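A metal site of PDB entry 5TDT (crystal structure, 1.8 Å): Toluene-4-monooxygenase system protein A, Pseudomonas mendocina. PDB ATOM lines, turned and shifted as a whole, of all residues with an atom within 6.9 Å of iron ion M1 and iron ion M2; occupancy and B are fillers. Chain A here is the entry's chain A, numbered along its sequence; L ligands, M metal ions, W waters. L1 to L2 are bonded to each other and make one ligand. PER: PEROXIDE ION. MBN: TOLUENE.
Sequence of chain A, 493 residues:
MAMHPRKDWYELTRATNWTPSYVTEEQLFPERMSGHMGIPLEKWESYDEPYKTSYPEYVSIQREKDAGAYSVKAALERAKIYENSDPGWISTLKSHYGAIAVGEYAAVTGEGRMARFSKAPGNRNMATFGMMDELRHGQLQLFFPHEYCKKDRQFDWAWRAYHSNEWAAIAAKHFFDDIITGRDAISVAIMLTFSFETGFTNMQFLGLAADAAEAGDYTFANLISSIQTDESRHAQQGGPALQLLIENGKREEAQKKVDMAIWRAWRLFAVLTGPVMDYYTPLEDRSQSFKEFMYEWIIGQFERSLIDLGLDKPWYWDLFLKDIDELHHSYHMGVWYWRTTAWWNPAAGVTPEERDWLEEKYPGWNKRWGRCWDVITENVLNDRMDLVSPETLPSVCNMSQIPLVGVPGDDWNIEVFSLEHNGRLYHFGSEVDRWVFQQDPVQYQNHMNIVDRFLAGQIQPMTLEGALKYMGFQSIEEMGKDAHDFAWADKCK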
ATOM      1  N   ILE A 100      29.353  24.647   6.898  1.00  0.00           N
ATOM      2  CA  ILE A 100      27.994  24.671   6.366  1.00  0.00           C
ATOM      3  C   ILE A 100      27.220  23.386   6.659  1.00  0.00           C
ATOM      4  O   ILE A 100      26.039  23.460   6.996  1.00  0.00           O
ATOM      5  CB  ILE A 100      28.023  24.984   4.852  1.00  0.00           C
ATOM      6  CG1 ILE A 100      28.525  26.412   4.585  1.00  0.00           C
ATOM      7  CG2 ILE A 100      26.637  24.768   4.215  1.00  0.00           C
ATOM      8  CD1 ILE A 100      27.733  27.500   5.283  1.00  0.00           C
ATOM      9  N   GLU A 104      23.442  23.363   8.067  1.00  0.00           N
ATOM     10  CA  GLU A 104      22.254  23.063   7.270  1.00  0.00           C
ATOM     11  C   GLU A 104      21.331  22.109   8.006  1.00  0.00           C
ATOM     12  O   GLU A 104      20.108  22.280   8.018  1.00  0.00           O
ATOM     13  CB  GLU A 104      22.661  22.453   5.929  1.00  0.00           C
ATOM     14  CG  GLU A 104      23.482  23.379   5.082  1.00  0.00           C
ATOM     15  CD  GLU A 104      22.677  24.038   3.989  1.00  0.00           C
ATOM     16  OE1 GLU A 104      23.272  24.352   2.939  1.00  0.00           O
ATOM     17  OE2 GLU A 104      21.441  24.219   4.167  1.00  0.00           O
ATOM     18  N   ALA A 107      19.343  23.850  10.445  1.00  0.00           N
ATOM     19  CA  ALA A 107      18.241  24.620   9.878  1.00  0.00           C
ATOM     20  C   ALA A 107      16.948  23.816   9.811  1.00  0.00           C
ATOM     21  O   ALA A 107      15.862  24.412   9.780  1.00  0.00           O
ATOM     22  CB  ALA A 107      18.615  25.144   8.485  1.00  0.00           C
ATOM     23  N   GLU A 111      13.137  25.376  10.696  1.00  0.00           N
ATOM     24  CA  GLU A 111      11.925  25.120   9.938  1.00  0.00           C
ATOM     25  C   GLU A 111      10.902  24.341  10.773  1.00  0.00           C
ATOM     26  O   GLU A 111       9.705  24.613  10.720  1.00  0.00           O
ATOM     27  CB  GLU A 111      12.267  24.343   8.652  1.00  0.00           C
ATOM     28  CG  GLU A 111      13.131  25.127   7.625  1.00  0.00           C
ATOM     29  CD  GLU A 111      12.370  26.224   6.871  1.00  0.00           C
ATOM     30  OE1 GLU A 111      11.126  26.295   6.977  1.00  0.00           O
ATOM     31  OE2 GLU A 111      13.032  27.018   6.135  1.00  0.00           O
ATOM     32  N   GLY A 130      10.296  23.113   3.953  1.00  0.00           N
ATOM     33  CA  GLY A 130      11.578  23.654   4.409  1.00  0.00           C
ATOM     34  C   GLY A 130      12.371  22.664   5.239  1.00  0.00           C
ATOM     35  O   GLY A 130      13.592  22.550   5.073  1.00  0.00           O
ATOM     36  N   ASP A 133      13.833  20.325   2.754  1.00  0.00           N
ATOM     37  CA  ASP A 133      14.931  20.952   2.007  1.00  0.00           C
ATOM     38  C   ASP A 133      16.222  20.924   2.812  1.00  0.00           C
ATOM     39  O   ASP A 133      17.298  20.608   2.272  1.00  0.00           O
ATOM     40  CB  ASP A 133      14.585  22.397   1.643  1.00  0.00           C
ATOM     41  CG  ASP A 133      13.455  22.523   0.641  1.00  0.00           C
ATOM     42  OD1 ASP A 133      13.094  21.535  -0.063  1.00  0.00           O
ATOM     43  OD2 ASP A 133      12.929  23.646   0.542  1.00  0.00           O
ATOM     44  N   GLU A 134      16.163  21.298   4.092  1.00  0.00           N
ATOM     45  CA  GLU A 134      17.424  21.399   4.825  1.00  0.00           C
ATOM     46  C   GLU A 134      17.972  20.012   5.164  1.00  0.00           C
ATOM     47  O   GLU A 134      19.189  19.846   5.285  1.00  0.00           O
ATOM     48  CB  GLU A 134      17.256  22.248   6.087  1.00  0.00           C
ATOM     49  CG  GLU A 134      16.673  23.646   5.835  1.00  0.00           C
ATOM     50  CD  GLU A 134      17.593  24.587   5.042  1.00  0.00           C
ATOM     51  OE1 GLU A 134      18.586  24.145   4.401  1.00  0.00           O
ATOM     52  OE2 GLU A 134      17.316  25.808   5.067  1.00  0.00           O
ATOM     53  N   HIS A 137      19.977  19.349   2.184  1.00  0.00           N
ATOM     54  CA  HIS A 137      21.212  20.116   2.117  1.00  0.00           C
ATOM     55  C   HIS A 137      22.264  19.581   3.085  1.00  0.00           C
ATOM     56  O   HIS A 137      23.448  19.523   2.741  1.00  0.00           O
ATOM     57  CB  HIS A 137      20.929  21.595   2.378  1.00  0.00           C
ATOM     58  CG  HIS A 137      19.944  22.183   1.419  1.00  0.00           C
ATOM     59  ND1 HIS A 137      19.365  23.422   1.591  1.00  0.00           N
ATOM     60  CD2 HIS A 137      19.438  21.688   0.261  1.00  0.00           C
ATOM     61  CE1 HIS A 137      18.536  23.666   0.589  1.00  0.00           C
ATOM     62  NE2 HIS A 137      18.560  22.625  -0.241  1.00  0.00           N
ATOM     63  N   GLY A 138      21.852  19.163   4.283  1.00  0.00           N
ATOM     64  CA  GLY A 138      22.813  18.599   5.213  1.00  0.00           C
ATOM     65  C   GLY A 138      23.320  17.250   4.759  1.00  0.00           C
ATOM     66  O   GLY A 138      24.503  16.942   4.923  1.00  0.00           O
ATOM     67  N   GLN A 141      25.741  17.718   1.739  1.00  0.00           N
ATOM     68  CA  GLN A 141      27.016  18.337   2.069  1.00  0.00           C
ATOM     69  C   GLN A 141      27.811  17.544   3.094  1.00  0.00           C
ATOM     70  O   GLN A 141      28.937  17.943   3.421  1.00  0.00           O
ATOM     71  CB  GLN A 141      26.774  19.777   2.502  1.00  0.00           C
ATOM     72  CG  GLN A 141      26.465  20.581   1.247  1.00  0.00           C
ATOM     73  CD  GLN A 141      26.009  21.977   1.508  1.00  0.00           C
ATOM     74  OE1 GLN A 141      26.654  22.938   1.060  1.00  0.00           O
ATOM     75  NE2 GLN A 141      24.880  22.121   2.184  1.00  0.00           N
ATOM     76  N   LEU A 192      16.047  34.096   9.808  1.00  0.00           N
ATOM     77  CA  LEU A 192      16.597  33.037   8.955  1.00  0.00           C
ATOM     78  C   LEU A 192      16.090  33.196   7.523  1.00  0.00           C
ATOM     79  O   LEU A 192      16.869  33.510   6.619  1.00  0.00           O
ATOM     80  CB  LEU A 192      16.234  31.662   9.511  1.00  0.00           C
ATOM     81  CG  LEU A 192      16.537  30.464   8.586  1.00  0.00           C
ATOM     82  CD1 LEU A 192      18.032  30.366   8.247  1.00  0.00           C
ATOM     83  CD2 LEU A 192      16.057  29.159   9.204  1.00  0.00           C
ATOM     84  N   THR A 193      14.785  32.978   7.294  1.00  0.00           N
ATOM     85  CA  THR A 193      14.345  32.829   5.907  1.00  0.00           C
ATOM     86  C   THR A 193      14.451  34.147   5.143  1.00  0.00           C
ATOM     87  O   THR A 193      14.904  34.158   3.989  1.00  0.00           O
ATOM     88  CB  THR A 193      12.930  32.236   5.824  1.00  0.00           C
ATOM     89  OG1 THR A 193      11.944  33.171   6.240  1.00  0.00           O
ATOM     90  CG2 THR A 193      12.826  30.968   6.666  1.00  0.00           C
ATOM     91  N   PHE A 196      18.847  36.036   6.318  1.00  0.00           N
ATOM     92  CA  PHE A 196      19.982  35.204   5.947  1.00  0.00           C
ATOM     93  C   PHE A 196      19.762  34.525   4.587  1.00  0.00           C
ATOM     94  O   PHE A 196      20.655  34.523   3.734  1.00  0.00           O
ATOM     95  CB  PHE A 196      20.221  34.168   7.035  1.00  0.00           C
ATOM     96  CG  PHE A 196      21.408  33.288   6.809  1.00  0.00           C
ATOM     97  CD1 PHE A 196      22.684  33.847   6.736  1.00  0.00           C
ATOM     98  CD2 PHE A 196      21.265  31.917   6.699  1.00  0.00           C
ATOM     99  CE1 PHE A 196      23.795  33.025   6.524  1.00  0.00           C
ATOM    100  CE2 PHE A 196      22.361  31.109   6.495  1.00  0.00           C
ATOM    101  CZ  PHE A 196      23.628  31.657   6.410  1.00  0.00           C
ATOM    102  N   GLU A 197      18.560  33.974   4.354  1.00  0.00           N
ATOM    103  CA  GLU A 197      18.350  33.079   3.219  1.00  0.00           C
ATOM    104  C   GLU A 197      17.992  33.797   1.909  1.00  0.00           C
ATOM    105  O   GLU A 197      18.210  33.210   0.838  1.00  0.00           O
ATOM    106  CB  GLU A 197      17.283  32.040   3.539  1.00  0.00           C
ATOM    107  CG  GLU A 197      17.756  31.037   4.609  1.00  0.00           C
ATOM    108  CD  GLU A 197      16.806  29.869   4.841  1.00  0.00           C
ATOM    109  OE1 GLU A 197      15.578  30.068   4.893  1.00  0.00           O
ATOM    110  OE2 GLU A 197      17.288  28.730   4.969  1.00  0.00           O
ATOM    111  N   THR A 201      23.113  34.005   1.836  1.00  0.00           N
ATOM    112  CA  THR A 201      23.547  32.709   1.320  1.00  0.00           C
ATOM    113  C   THR A 201      23.852  32.751  -0.172  1.00  0.00           C
ATOM    114  O   THR A 201      24.628  31.931  -0.672  1.00  0.00           O
ATOM    115  CB  THR A 201      22.521  31.609   1.602  1.00  0.00           C
ATOM    116  OG1 THR A 201      21.254  31.988   1.051  1.00  0.00           O
ATOM    117  CG2 THR A 201      22.385  31.372   3.112  1.00  0.00           C
ATOM    118  N   PHE A 205      26.684  30.404  -2.006  1.00  0.00           N
ATOM    119  CA  PHE A 205      26.179  29.324  -2.839  1.00  0.00           C
ATOM    120  C   PHE A 205      26.067  29.674  -4.317  1.00  0.00           C
ATOM    121  O   PHE A 205      25.864  28.764  -5.137  1.00  0.00           O
ATOM    122  CB  PHE A 205      24.810  28.850  -2.332  1.00  0.00           C
ATOM    123  CG  PHE A 205      24.892  28.043  -1.073  1.00  0.00           C
ATOM    124  CD1 PHE A 205      25.069  28.677   0.156  1.00  0.00           C
ATOM    125  CD2 PHE A 205      24.806  26.665  -1.114  1.00  0.00           C
ATOM    126  CE1 PHE A 205      25.139  27.927   1.338  1.00  0.00           C
ATOM    127  CE2 PHE A 205      24.885  25.913   0.054  1.00  0.00           C
ATOM    128  CZ  PHE A 205      25.059  26.556   1.287  1.00  0.00           C
ATOM    129  N   ILE A 227      21.371  23.368  -4.634  1.00  0.00           N
ATOM    130  CA  ILE A 227      20.912  23.629  -3.283  1.00  0.00           C
ATOM    131  C   ILE A 227      20.206  24.980  -3.228  1.00  0.00           C
ATOM    132  O   ILE A 227      19.130  25.127  -2.629  1.00  0.00           O
ATOM    133  CB  ILE A 227      22.113  23.554  -2.318  1.00  0.00           C
ATOM    134  CG1 ILE A 227      22.493  22.085  -2.098  1.00  0.00           C
ATOM    135  CG2 ILE A 227      21.821  24.296  -1.011  1.00  0.00           C
ATOM    136  CD1 ILE A 227      23.799  21.903  -1.319  1.00  0.00           C
ATOM    137  N   GLN A 228      20.765  25.994  -3.896  1.00  0.00           N
ATOM    138  CA  GLN A 228      20.187  27.320  -3.774  1.00  0.00           C
ATOM    139  C   GLN A 228      18.827  27.425  -4.464  1.00  0.00           C
ATOM    140  O   GLN A 228      18.053  28.319  -4.126  1.00  0.00           O
ATOM    141  CB  GLN A 228      21.156  28.393  -4.306  1.00  0.00           C
ATOM    142  CG  GLN A 228      20.933  29.827  -3.751  1.00  0.00           C
ATOM    143  CD  GLN A 228      21.263  29.970  -2.241  1.00  0.00           C
ATOM    144  OE1 GLN A 228      21.499  28.990  -1.544  1.00  0.00           O
ATOM    145  NE2 GLN A 228      21.275  31.201  -1.763  1.00  0.00           N
ATOM    146  N   ASP A 230      16.444  25.319  -3.895  1.00  0.00           N
ATOM    147  CA  ASP A 230      15.543  25.090  -2.763  1.00  0.00           C
ATOM    148  C   ASP A 230      15.443  26.334  -1.888  1.00  0.00           C
ATOM    149  O   ASP A 230      14.347  26.716  -1.452  1.00  0.00           O
ATOM    150  CB  ASP A 230      16.021  23.897  -1.900  1.00  0.00           C
ATOM    151  CG  ASP A 230      16.129  22.585  -2.679  1.00  0.00           C
ATOM    152  OD1 ASP A 230      17.074  21.834  -2.399  1.00  0.00           O
ATOM    153  OD2 ASP A 230      15.269  22.308  -3.555  1.00  0.00           O
ATOM    154  N   GLU A 231      16.597  26.908  -1.550  1.00  0.00           N
ATOM    155  CA  GLU A 231      16.640  28.126  -0.740  1.00  0.00           C
ATOM    156  C   GLU A 231      15.704  29.181  -1.310  1.00  0.00           C
ATOM    157  O   GLU A 231      14.932  29.809  -0.566  1.00  0.00           O
ATOM    158  CB  GLU A 231      18.079  28.648  -0.683  1.00  0.00           C
ATOM    159  CG  GLU A 231      18.244  29.897   0.158  1.00  0.00           C
ATOM    160  CD  GLU A 231      18.577  29.582   1.600  1.00  0.00           C
ATOM    161  OE1 GLU A 231      19.638  30.033   2.087  1.00  0.00           O
ATOM    162  OE2 GLU A 231      17.781  28.869   2.233  1.00  0.00           O
ATOM    163  N   SER A 232      15.745  29.375  -2.616  1.00  0.00           N
ATOM    164  CA  SER A 232      14.965  30.430  -3.248  1.00  0.00           C
ATOM    165  C   SER A 232      13.467  30.235  -3.003  1.00  0.00           C
ATOM    166  O   SER A 232      12.736  31.209  -2.899  1.00  0.00           O
ATOM    167  CB  SER A 232      15.288  30.509  -4.734  1.00  0.00           C
ATOM    168  OG  SER A 232      16.634  30.897  -4.885  1.00  0.00           O
ATOM    169  N   HIS A 234      11.997  28.225  -0.166  1.00  0.00           N
ATOM    170  CA  HIS A 234      11.542  28.302   1.228  1.00  0.00           C
ATOM    171  C   HIS A 234      11.971  29.601   1.918  1.00  0.00           C
ATOM    172  O   HIS A 234      11.375  29.948   2.943  1.00  0.00           O
ATOM    173  CB  HIS A 234      11.977  27.065   2.047  1.00  0.00           C
ATOM    174  CG  HIS A 234      13.448  26.927   2.270  1.00  0.00           C
ATOM    175  ND1 HIS A 234      14.154  25.806   1.874  1.00  0.00           N
ATOM    176  CD2 HIS A 234      14.340  27.717   2.921  1.00  0.00           C
ATOM    177  CE1 HIS A 234      15.426  25.933   2.225  1.00  0.00           C
ATOM    178  NE2 HIS A 234      15.557  27.088   2.865  1.00  0.00           N
ATOM    179  N   ALA A 235      12.929  30.343   1.358  1.00  0.00           N
ATOM    180  CA  ALA A 235      13.211  31.675   1.882  1.00  0.00           C
ATOM    181  C   ALA A 235      12.030  32.636   1.691  1.00  0.00           C
ATOM    182  O   ALA A 235      11.935  33.626   2.407  1.00  0.00           O
ATOM    183  CB  ALA A 235      14.464  32.276   1.227  1.00  0.00           C
HETATM  184  O1  PER L   1      20.413  27.220   4.232  1.00  0.00           O
HETATM  185  O2  PER L   1      19.669  26.594   5.252  1.00  0.00           O
HETATM  186  C   MBN L   2      24.730  26.772   7.287  1.00  0.00           C
HETATM  187  C1  MBN L   2      23.457  27.159   6.558  1.00  0.00           C
HETATM  188  C2  MBN L   2      22.265  27.148   7.260  1.00  0.00           C
HETATM  189  C3  MBN L   2      21.100  27.509   6.614  1.00  0.00           C
HETATM  190  C4  MBN L   2      21.104  27.832   5.258  1.00  0.00           C
HETATM  191  C5  MBN L   2      22.311  27.836   4.561  1.00  0.00           C
HETATM  192  C6  MBN L   2      23.487  27.499   5.212  1.00  0.00           C
HETATM  193 FE    FE M   1      17.674  27.350   3.648  1.00  0.00          FE
HETATM  194 FE    FE M   2      19.890  25.029   3.074  1.00  0.00          FE
HETATM  195  O   HOH W   1      21.317  25.740   1.816  1.00  0.00           O
HETATM  196  O   HOH W   2      18.523  26.427   2.210  1.00  0.00           O
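Four residues have an atom within 4 Å of iron ion M1: Glu 134, Glu 197, Glu 231 and His 234.
Iron ion M2 is bound by water W1 (2.0 Å), the side-chain carboxylate (OE1) of Glu 134 (2.1 Å), the side-chain carboxylate (OE2) of Glu 104 (2.1 Å), water W2 (2.1 Å), a ring nitrogen (ND1) of His 137 (2.2 Å) and an oxygen (O1) of PER L1 (2.5 Å).
O of Leu 192 is in hydrogen-bond range of N of Glu 197 (2.9 Å).
O of Glu 197 is in hydrogen-bond range of OG1 of Thr 201 (3.3 Å).
The side-chain carboxylate (OE1) of Glu 104 sits at hydrogen-bond distance from the side-chain amide nitrogen (NE2) of Gln 141.
The side-chain carboxylate (OE1) of Glu 231 is in hydrogen-bond range of the side-chain hydroxyl (OG1) of Thr 201 (2.7 Å).
NE2 of His 137 sits close to O of Asp 133 (3.5 Å).
NE2 of His 137 lies within hydrogen-bond range of OD1 of Asp 230, 2.7 Å away.
A ring nitrogen (ND1) of His 234 lies within hydrogen-bond range of the side-chain carboxylate of Asp 133 (2.8 Å).
O of Asp 230 sits at hydrogen-bond distance from ND1 of His 234, at 3.5 Å.
Iron ion M1 is bound by water W2 (1.9 Å).
OE2 of Glu 197 binds iron ion M1 (1.9 Å).
Iron ion M1 is bound by OE2 of Glu 231, 2.1 Å away.
Iron ion M1 is bound by OE2 of Glu 134, 2.1 Å away.
A ring nitrogen (NE2) of His 234 is bound to iron ion M1, at 2.3 Å.
Slightly farther from iron ion M1 lies an oxygen (O2) of PER L1 (2.7 Å).
The nearest printed residue that does not touch iron ion M2 is Glu 231 (4.5 Å).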
